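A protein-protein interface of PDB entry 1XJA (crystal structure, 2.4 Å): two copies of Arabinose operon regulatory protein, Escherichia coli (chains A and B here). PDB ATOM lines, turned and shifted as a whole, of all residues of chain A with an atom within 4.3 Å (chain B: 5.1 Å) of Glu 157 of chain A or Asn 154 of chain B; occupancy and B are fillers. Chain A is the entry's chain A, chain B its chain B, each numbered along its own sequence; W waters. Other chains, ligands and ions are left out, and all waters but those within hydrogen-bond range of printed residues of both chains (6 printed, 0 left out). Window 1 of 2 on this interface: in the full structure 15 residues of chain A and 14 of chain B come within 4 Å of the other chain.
The side-chain amide oxygen (OD1) of Asn 154 of chain A lies close to the backbone carbonyl oxygen (O) of Asn 154 of chain B, at 3.0 Å.
OH of Tyr 103 of chain A is in hydrogen-bond range of NE of Arg 101 of chain B.
The side-chain hydroxyl (OH) of Tyr 103 of chain A is in hydrogen-bond range of the side-chain hydroxyl (OH) of Tyr 103 of chain B, at 3.1 Å.
OE2 of Glu 157 of chain A sits close to OD1 of Asn 154 of chain B (3.1 Å).
OD1 of Asn 154 of chain A is in hydrogen-bond range of N of Gln 158 of chain B (3.5 Å).
OD1 of Asn 154 of chain A lies close to OE2 of Glu 157 of chain B (3.1 Å).
The side-chain hydroxyl (OH) of Tyr 103 of chain B sits at hydrogen-bond distance from the guanidinium group (NE) of Arg 101 of chain A (3.4 Å).
The side-chain hydroxyl of Tyr 103 of chain A is in hydrogen-bond range of the side-chain carboxylate of Glu 157 of chain A, at 2.6 Å.
The indole nitrogen of Trp 104 of chain A lies within hydrogen-bond range of the side-chain carboxylate of Glu 157 of chain A.
OH of Tyr 103 of chain B lies within hydrogen-bond range of OE1 of Glu 157 of chain B, 2.6 Å away.
Among the printed residues, merely in contact across the chains: Leu 155 of chain A with Gln 158 of chain B, Gln 158 of chain A with Asn 154 of chain B, Gln 158 of chain A with Gln 158 of chain B and Leu 161 of chain A with Leu 150 of chain B.
Ile 153 of chain A touches none of the printed residues of chain B.
Glu 157 of chain A touches just one residue of chain B: Asn 154 (3.1 Å).
Of the printed residues of chain B, Leu 161 of chain A touches Leu 150 (3.6 Å).
Of the printed residues of chain A, Tyr 103 of chain B touches Arg 101 (3.4 Å) and Tyr 103 (3.1 Å).
Glu 149 of chain B touches none of the printed residues of chain A.
Of the printed residues of chain A, Asn 154 of chain B touches Asn 154, Glu 157 and Gln 158.
Printed residues of chain A within 4 Å of Glu 157 of chain B: Asn 154.
Printed residues of chain A within 4 Å of Gln 158 of chain B: Asn 154, Leu 155 and Gln 158.
The nearest printed residue of chain A that does not touch Leu 150 of chain B is Glu 157 of chain A (4.9 Å).
Of the 12 printed residues of chain A, 7 touch a printed residue of chain B.
Hydrophobic or aromatic side chains of chain A within 4 Å of the printed part of chain B: Tyr 103, Leu 155 and Leu 161.
Along chain A the printed residues that touch a printed residue of chain B span positions 101 to 161.
Arg 101 of chain A touches Tyr 103 of chain B, and with the chains exchanged Tyr 103 of chain A touches Arg 101 of chain B.
Tyr 103 of chain B touches its own counterpart, Tyr 103 of chain A.
Leu 155 of chain A touches Gln 158 of chain B, but with the chains exchanged Gln 158 of chain A does not touch Leu 155 of chain B (4.1 Å).
Gln 158 of chain A touches its own counterpart, Gln 158 of chain B.
Water W3 lies within hydrogen-bond range of ND2 of Asn 154 of chain B (2.6 Å), ND2 of Asn 154 of chain A (2.6 Å), OE1 of Gln 158 of chain A (2.8 Å) and OE1 of Gln 158 of chain B (2.9 Å).
Water W4 lies within hydrogen-bond range of the side-chain carboxylate of Glu 157 of chain A (2.7 Å), the guanidinium group of Arg 101 of chain B (2.9 Å) and the side-chain carboxylate of Glu 157 of chain B (3.1 Å).
Water W2 lies within hydrogen-bond range of OE2 of Glu 157 of chain A (2.7 Å), O of Leu 150 of chain B (2.8 Å) and NH2 of Arg 101 of chain B (3.1 Å).
Water W6 lies within hydrogen-bond range of OE1 of Glu 157 of chain A, NE of Arg 101 of chain A and OE2 of Glu 157 of chain B.
Water W1 lies within hydrogen-bond range of OE2 of Glu 157 of chain B (2.9 Å) and NH2 of Arg 101 of chain A (2.9 Å).
Water W5 bridges the side-chain amide oxygen of Gln 158 of chain B and the side-chain amide oxygen of Gln 158 of chain A.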
ATOM      1  N   ARG A 101      -6.336  32.654  -1.213  1.00  0.00           N
ATOM      2  CA  ARG A 101      -7.382  33.137  -2.096  1.00  0.00           C
ATOM      3  C   ARG A 101      -7.947  34.276  -1.251  1.00  0.00           C
ATOM      4  O   ARG A 101      -7.830  34.264  -0.018  1.00  0.00           O
ATOM      5  CB  ARG A 101      -8.447  32.064  -2.339  1.00  0.00           C
ATOM      6  CG  ARG A 101      -7.985  30.899  -3.229  1.00  0.00           C
ATOM      7  CD  ARG A 101      -9.150  29.972  -3.555  1.00  0.00           C
ATOM      8  NE  ARG A 101      -8.820  28.875  -4.469  1.00  0.00           N
ATOM      9  CZ  ARG A 101      -8.516  29.020  -5.758  1.00  0.00           C
ATOM     10  NH1 ARG A 101      -8.488  30.230  -6.303  1.00  0.00           N
ATOM     11  NH2 ARG A 101      -8.260  27.952  -6.513  1.00  0.00           N
ATOM     12  N   TYR A 103     -10.898  35.133  -0.150  1.00  0.00           N
ATOM     13  CA  TYR A 103     -11.844  34.819   0.917  1.00  0.00           C
ATOM     14  C   TYR A 103     -11.346  33.944   2.069  1.00  0.00           C
ATOM     15  O   TYR A 103     -12.131  33.567   2.942  1.00  0.00           O
ATOM     16  CB  TYR A 103     -13.119  34.221   0.315  1.00  0.00           C
ATOM     17  CG  TYR A 103     -12.919  32.956  -0.484  1.00  0.00           C
ATOM     18  CD1 TYR A 103     -12.903  31.713   0.142  1.00  0.00           C
ATOM     19  CD2 TYR A 103     -12.752  32.998  -1.877  1.00  0.00           C
ATOM     20  CE1 TYR A 103     -12.731  30.537  -0.584  1.00  0.00           C
ATOM     21  CE2 TYR A 103     -12.574  31.818  -2.619  1.00  0.00           C
ATOM     22  CZ  TYR A 103     -12.565  30.591  -1.957  1.00  0.00           C
ATOM     23  OH  TYR A 103     -12.364  29.414  -2.649  1.00  0.00           O
ATOM     24  N   TRP A 104     -10.050  33.643   2.092  1.00  0.00           N
ATOM     25  CA  TRP A 104      -9.476  32.816   3.159  1.00  0.00           C
ATOM     26  C   TRP A 104      -9.094  33.604   4.411  1.00  0.00           C
ATOM     27  O   TRP A 104      -9.010  33.035   5.495  1.00  0.00           O
ATOM     28  CB  TRP A 104      -8.208  32.089   2.672  1.00  0.00           C
ATOM     29  CG  TRP A 104      -8.415  30.968   1.693  1.00  0.00           C
ATOM     30  CD1 TRP A 104      -9.590  30.580   1.127  1.00  0.00           C
ATOM     31  CD2 TRP A 104      -7.403  30.105   1.147  1.00  0.00           C
ATOM     32  NE1 TRP A 104      -9.378  29.534   0.260  1.00  0.00           N
ATOM     33  CE2 TRP A 104      -8.044  29.222   0.254  1.00  0.00           C
ATOM     34  CE3 TRP A 104      -6.014  29.997   1.328  1.00  0.00           C
ATOM     35  CZ2 TRP A 104      -7.347  28.236  -0.463  1.00  0.00           C
ATOM     36  CZ3 TRP A 104      -5.323  29.022   0.616  1.00  0.00           C
ATOM     37  CH2 TRP A 104      -5.995  28.152  -0.272  1.00  0.00           C
ATOM     38  N   ILE A 153      -4.212  23.596  -3.334  1.00  0.00           N
ATOM     39  CA  ILE A 153      -4.885  24.797  -2.862  1.00  0.00           C
ATOM     40  C   ILE A 153      -6.252  24.421  -2.306  1.00  0.00           C
ATOM     41  O   ILE A 153      -6.714  24.986  -1.317  1.00  0.00           O
ATOM     42  CB  ILE A 153      -5.083  25.784  -4.003  1.00  0.00           C
ATOM     43  CG1 ILE A 153      -3.725  26.266  -4.504  1.00  0.00           C
ATOM     44  CG2 ILE A 153      -5.942  26.944  -3.544  1.00  0.00           C
ATOM     45  CD1 ILE A 153      -2.987  27.109  -3.511  1.00  0.00           C
ATOM     46  N   ASN A 154      -6.896  23.462  -2.959  1.00  0.00           N
ATOM     47  CA  ASN A 154      -8.208  22.992  -2.546  1.00  0.00           C
ATOM     48  C   ASN A 154      -8.100  22.306  -1.192  1.00  0.00           C
ATOM     49  O   ASN A 154      -8.905  22.546  -0.292  1.00  0.00           O
ATOM     50  CB  ASN A 154      -8.750  21.994  -3.569  1.00  0.00           C
ATOM     51  CG  ASN A 154     -10.052  21.358  -3.130  1.00  0.00           C
ATOM     52  OD1 ASN A 154     -11.122  21.957  -3.242  1.00  0.00           O
ATOM     53  ND2 ASN A 154      -9.966  20.139  -2.616  1.00  0.00           N
ATOM     54  N   LEU A 155      -7.098  21.447  -1.057  1.00  0.00           N
ATOM     55  CA  LEU A 155      -6.897  20.718   0.179  1.00  0.00           C
ATOM     56  C   LEU A 155      -6.518  21.664   1.315  1.00  0.00           C
ATOM     57  O   LEU A 155      -6.907  21.444   2.463  1.00  0.00           O
ATOM     58  CB  LEU A 155      -5.832  19.639  -0.020  1.00  0.00           C
ATOM     59  CG  LEU A 155      -6.288  18.535  -0.979  1.00  0.00           C
ATOM     60  CD1 LEU A 155      -5.295  17.375  -0.964  1.00  0.00           C
ATOM     61  CD2 LEU A 155      -7.657  18.046  -0.557  1.00  0.00           C
ATOM     62  N   LEU A 156      -5.766  22.715   0.997  1.00  0.00           N
ATOM     63  CA  LEU A 156      -5.380  23.690   2.006  1.00  0.00           C
ATOM     64  C   LEU A 156      -6.644  24.402   2.487  1.00  0.00           C
ATOM     65  O   LEU A 156      -6.809  24.667   3.685  1.00  0.00           O
ATOM     66  CB  LEU A 156      -4.394  24.707   1.424  1.00  0.00           C
ATOM     67  CG  LEU A 156      -4.029  25.885   2.332  1.00  0.00           C
ATOM     68  CD1 LEU A 156      -3.704  25.380   3.733  1.00  0.00           C
ATOM     69  CD2 LEU A 156      -2.848  26.634   1.759  1.00  0.00           C
ATOM     70  N   GLU A 157      -7.540  24.699   1.547  1.00  0.00           N
ATOM     71  CA  GLU A 157      -8.789  25.371   1.878  1.00  0.00           C
ATOM     72  C   GLU A 157      -9.578  24.455   2.789  1.00  0.00           C
ATOM     73  O   GLU A 157     -10.243  24.914   3.720  1.00  0.00           O
ATOM     74  CB  GLU A 157      -9.605  25.675   0.615  1.00  0.00           C
ATOM     75  CG  GLU A 157     -10.997  26.238   0.883  1.00  0.00           C
ATOM     76  CD  GLU A 157     -11.728  26.640  -0.392  1.00  0.00           C
ATOM     77  OE1 GLU A 157     -11.274  27.588  -1.073  1.00  0.00           O
ATOM     78  OE2 GLU A 157     -12.756  26.006  -0.714  1.00  0.00           O
ATOM     79  N   GLN A 158      -9.497  23.154   2.527  1.00  0.00           N
ATOM     80  CA  GLN A 158     -10.215  22.196   3.362  1.00  0.00           C
ATOM     81  C   GLN A 158      -9.664  22.244   4.782  1.00  0.00           C
ATOM     82  O   GLN A 158     -10.414  22.360   5.752  1.00  0.00           O
ATOM     83  CB  GLN A 158     -10.079  20.765   2.827  1.00  0.00           C
ATOM     84  CG  GLN A 158     -11.095  19.815   3.457  1.00  0.00           C
ATOM     85  CD  GLN A 158     -10.852  18.356   3.109  1.00  0.00           C
ATOM     86  OE1 GLN A 158     -10.579  18.012   1.954  1.00  0.00           O
ATOM     87  NE2 GLN A 158     -10.969  17.488   4.105  1.00  0.00           N
ATOM     88  N   LEU A 159      -8.347  22.161   4.892  1.00  0.00           N
ATOM     89  CA  LEU A 159      -7.696  22.189   6.192  1.00  0.00           C
ATOM     90  C   LEU A 159      -8.110  23.415   7.000  1.00  0.00           C
ATOM     91  O   LEU A 159      -8.464  23.294   8.172  1.00  0.00           O
ATOM     92  CB  LEU A 159      -6.171  22.160   6.021  1.00  0.00           C
ATOM     93  CG  LEU A 159      -5.385  21.780   7.283  1.00  0.00           C
ATOM     94  CD1 LEU A 159      -4.155  20.959   6.902  1.00  0.00           C
ATOM     95  CD2 LEU A 159      -5.002  23.030   8.049  1.00  0.00           C
ATOM     96  N   LEU A 160      -8.074  24.592   6.379  1.00  0.00           N
ATOM     97  CA  LEU A 160      -8.460  25.810   7.080  1.00  0.00           C
ATOM     98  C   LEU A 160      -9.922  25.735   7.526  1.00  0.00           C
ATOM     99  O   LEU A 160     -10.268  26.169   8.621  1.00  0.00           O
ATOM    100  CB  LEU A 160      -8.262  27.035   6.185  1.00  0.00           C
ATOM    101  CG  LEU A 160      -6.846  27.459   5.781  1.00  0.00           C
ATOM    102  CD1 LEU A 160      -6.926  28.623   4.801  1.00  0.00           C
ATOM    103  CD2 LEU A 160      -6.053  27.845   7.013  1.00  0.00           C
ATOM    104  N   LEU A 161     -10.783  25.189   6.676  1.00  0.00           N
ATOM    105  CA  LEU A 161     -12.193  25.076   7.027  1.00  0.00           C
ATOM    106  C   LEU A 161     -12.435  24.051   8.135  1.00  0.00           C
ATOM    107  O   LEU A 161     -13.322  24.238   8.986  1.00  0.00           O
ATOM    108  CB  LEU A 161     -13.024  24.718   5.794  1.00  0.00           C
ATOM    109  CG  LEU A 161     -13.138  25.852   4.774  1.00  0.00           C
ATOM    110  CD1 LEU A 161     -13.926  25.394   3.551  1.00  0.00           C
ATOM    111  CD2 LEU A 161     -13.820  27.037   5.435  1.00  0.00           C
ATOM    112  N   ARG B 101     -18.234  28.931  -8.249  1.00  0.00           N
ATOM    113  CA  ARG B 101     -17.329  30.048  -7.977  1.00  0.00           C
ATOM    114  C   ARG B 101     -16.825  30.479  -9.340  1.00  0.00           C
ATOM    115  O   ARG B 101     -16.691  29.646 -10.234  1.00  0.00           O
ATOM    116  CB  ARG B 101     -16.144  29.603  -7.109  1.00  0.00           C
ATOM    117  CG  ARG B 101     -16.468  29.298  -5.651  1.00  0.00           C
ATOM    118  CD  ARG B 101     -15.194  28.943  -4.922  1.00  0.00           C
ATOM    119  NE  ARG B 101     -15.408  28.605  -3.518  1.00  0.00           N
ATOM    120  CZ  ARG B 101     -15.841  29.452  -2.593  1.00  0.00           C
ATOM    121  NH1 ARG B 101     -16.119  30.708  -2.912  1.00  0.00           N
ATOM    122  NH2 ARG B 101     -15.987  29.041  -1.340  1.00  0.00           N
ATOM    123  N   TYR B 103     -14.032  31.067 -10.921  1.00  0.00           N
ATOM    124  CA  TYR B 103     -13.006  30.262 -11.593  1.00  0.00           C
ATOM    125  C   TYR B 103     -13.329  28.775 -11.811  1.00  0.00           C
ATOM    126  O   TYR B 103     -12.492  28.036 -12.325  1.00  0.00           O
ATOM    127  CB  TYR B 103     -11.672  30.368 -10.833  1.00  0.00           C
ATOM    128  CG  TYR B 103     -11.714  29.844  -9.408  1.00  0.00           C
ATOM    129  CD1 TYR B 103     -12.149  30.651  -8.358  1.00  0.00           C
ATOM    130  CD2 TYR B 103     -11.353  28.523  -9.117  1.00  0.00           C
ATOM    131  CE1 TYR B 103     -12.230  30.153  -7.049  1.00  0.00           C
ATOM    132  CE2 TYR B 103     -11.433  28.014  -7.811  1.00  0.00           C
ATOM    133  CZ  TYR B 103     -11.873  28.835  -6.786  1.00  0.00           C
ATOM    134  OH  TYR B 103     -11.982  28.334  -5.507  1.00  0.00           O
ATOM    135  N   GLU B 149     -21.854  24.364   4.663  1.00  0.00           N
ATOM    136  CA  GLU B 149     -21.998  24.711   3.258  1.00  0.00           C
ATOM    137  C   GLU B 149     -20.651  24.980   2.596  1.00  0.00           C
ATOM    138  O   GLU B 149     -20.413  24.561   1.458  1.00  0.00           O
ATOM    139  CB  GLU B 149     -22.927  25.924   3.106  1.00  0.00           C
ATOM    140  CG  GLU B 149     -23.114  26.379   1.663  1.00  0.00           C
ATOM    141  CD  GLU B 149     -24.102  27.512   1.544  1.00  0.00           C
ATOM    142  OE1 GLU B 149     -24.066  28.420   2.406  1.00  0.00           O
ATOM    143  OE2 GLU B 149     -24.904  27.500   0.585  1.00  0.00           O
ATOM    144  N   LEU B 150     -19.767  25.673   3.308  1.00  0.00           N
ATOM    145  CA  LEU B 150     -18.441  25.975   2.776  1.00  0.00           C
ATOM    146  C   LEU B 150     -17.644  24.690   2.555  1.00  0.00           C
ATOM    147  O   LEU B 150     -16.826  24.604   1.640  1.00  0.00           O
ATOM    148  CB  LEU B 150     -17.695  26.905   3.727  1.00  0.00           C
ATOM    149  CG  LEU B 150     -18.256  28.330   3.795  1.00  0.00           C
ATOM    150  CD1 LEU B 150     -17.633  29.075   4.961  1.00  0.00           C
ATOM    151  CD2 LEU B 150     -17.992  29.051   2.481  1.00  0.00           C
ATOM    152  N   LEU B 151     -17.884  23.686   3.390  1.00  0.00           N
ATOM    153  CA  LEU B 151     -17.181  22.418   3.238  1.00  0.00           C
ATOM    154  C   LEU B 151     -17.680  21.699   1.995  1.00  0.00           C
ATOM    155  O   LEU B 151     -16.893  21.169   1.212  1.00  0.00           O
ATOM    156  CB  LEU B 151     -17.391  21.523   4.465  1.00  0.00           C
ATOM    157  CG  LEU B 151     -16.320  21.581   5.555  1.00  0.00           C
ATOM    158  CD1 LEU B 151     -16.727  20.692   6.723  1.00  0.00           C
ATOM    159  CD2 LEU B 151     -14.985  21.112   4.976  1.00  0.00           C
ATOM    160  N   ALA B 152     -18.997  21.686   1.819  1.00  0.00           N
ATOM    161  CA  ALA B 152     -19.613  21.036   0.670  1.00  0.00           C
ATOM    162  C   ALA B 152     -19.087  21.685  -0.602  1.00  0.00           C
ATOM    163  O   ALA B 152     -18.757  20.996  -1.568  1.00  0.00           O
ATOM    164  CB  ALA B 152     -21.126  21.168   0.744  1.00  0.00           C
ATOM    165  N   ILE B 153     -19.004  23.015  -0.586  1.00  0.00           N
ATOM    166  CA  ILE B 153     -18.502  23.767  -1.727  1.00  0.00           C
ATOM    167  C   ILE B 153     -17.073  23.339  -2.018  1.00  0.00           C
ATOM    168  O   ILE B 153     -16.705  23.067  -3.167  1.00  0.00           O
ATOM    169  CB  ILE B 153     -18.541  25.291  -1.450  1.00  0.00           C
ATOM    170  CG1 ILE B 153     -19.996  25.761  -1.421  1.00  0.00           C
ATOM    171  CG2 ILE B 153     -17.759  26.047  -2.516  1.00  0.00           C
ATOM    172  CD1 ILE B 153     -20.169  27.248  -1.234  1.00  0.00           C
ATOM    173  N   ASN B 154     -16.271  23.278  -0.964  1.00  0.00           N
ATOM    174  CA  ASN B 154     -14.879  22.873  -1.078  1.00  0.00           C
ATOM    175  C   ASN B 154     -14.756  21.462  -1.640  1.00  0.00           C
ATOM    176  O   ASN B 154     -13.940  21.198  -2.529  1.00  0.00           O
ATOM    177  CB  ASN B 154     -14.216  22.900   0.291  1.00  0.00           C
ATOM    178  CG  ASN B 154     -12.813  22.370   0.254  1.00  0.00           C
ATOM    179  OD1 ASN B 154     -11.899  23.041  -0.227  1.00  0.00           O
ATOM    180  ND2 ASN B 154     -12.631  21.153   0.736  1.00  0.00           N
ATOM    181  N   LEU B 155     -15.553  20.549  -1.091  1.00  0.00           N
ATOM    182  CA  LEU B 155     -15.531  19.165  -1.533  1.00  0.00           C
ATOM    183  C   LEU B 155     -16.012  19.055  -2.984  1.00  0.00           C
ATOM    184  O   LEU B 155     -15.487  18.258  -3.761  1.00  0.00           O
ATOM    185  CB  LEU B 155     -16.387  18.311  -0.602  1.00  0.00           C
ATOM    186  CG  LEU B 155     -15.811  18.139   0.806  1.00  0.00           C
ATOM    187  CD1 LEU B 155     -16.737  17.268   1.629  1.00  0.00           C
ATOM    188  CD2 LEU B 155     -14.430  17.493   0.732  1.00  0.00           C
ATOM    189  N   LEU B 156     -17.007  19.859  -3.347  1.00  0.00           N
ATOM    190  CA  LEU B 156     -17.497  19.857  -4.721  1.00  0.00           C
ATOM    191  C   LEU B 156     -16.341  20.254  -5.634  1.00  0.00           C
ATOM    192  O   LEU B 156     -16.120  19.627  -6.669  1.00  0.00           O
ATOM    193  CB  LEU B 156     -18.660  20.848  -4.894  1.00  0.00           C
ATOM    194  CG  LEU B 156     -19.090  21.137  -6.340  1.00  0.00           C
ATOM    195  CD1 LEU B 156     -19.264  19.829  -7.104  1.00  0.00           C
ATOM    196  CD2 LEU B 156     -20.387  21.945  -6.337  1.00  0.00           C
ATOM    197  N   GLU B 157     -15.606  21.293  -5.239  1.00  0.00           N
ATOM    198  CA  GLU B 157     -14.466  21.760  -6.016  1.00  0.00           C
ATOM    199  C   GLU B 157     -13.434  20.651  -6.151  1.00  0.00           C
ATOM    200  O   GLU B 157     -12.832  20.476  -7.207  1.00  0.00           O
ATOM    201  CB  GLU B 157     -13.815  22.987  -5.361  1.00  0.00           C
ATOM    202  CG  GLU B 157     -12.548  23.455  -6.075  1.00  0.00           C
ATOM    203  CD  GLU B 157     -11.920  24.692  -5.445  1.00  0.00           C
ATOM    204  OE1 GLU B 157     -12.499  25.795  -5.585  1.00  0.00           O
ATOM    205  OE2 GLU B 157     -10.844  24.561  -4.808  1.00  0.00           O
ATOM    206  N   GLN B 158     -13.222  19.897  -5.080  1.00  0.00           N
ATOM    207  CA  GLN B 158     -12.247  18.814  -5.140  1.00  0.00           C
ATOM    208  C   GLN B 158     -12.723  17.776  -6.156  1.00  0.00           C
ATOM    209  O   GLN B 158     -11.937  17.270  -6.950  1.00  0.00           O
ATOM    210  CB  GLN B 158     -12.075  18.146  -3.765  1.00  0.00           C
ATOM    211  CG  GLN B 158     -10.861  17.225  -3.687  1.00  0.00           C
ATOM    212  CD  GLN B 158     -10.912  16.283  -2.509  1.00  0.00           C
ATOM    213  OE1 GLN B 158     -11.139  16.702  -1.370  1.00  0.00           O
ATOM    214  NE2 GLN B 158     -10.692  14.996  -2.768  1.00  0.00           N
HETATM  215  O   HOH W   1      -8.348  25.059  -6.111  1.00  0.00           O
HETATM  216  O   HOH W   2     -15.251  26.484   0.239  1.00  0.00           O
HETATM  217  O   HOH W   3     -11.150  19.430  -0.441  1.00  0.00           O
HETATM  218  O   HOH W   4     -14.209  26.036  -2.976  1.00  0.00           O
HETATM  219  O   HOH W   5     -10.558  15.140   1.106  1.00  0.00           O
HETATM  220  O   HOH W   6      -9.589  26.476  -2.914  1.00  0.00           O
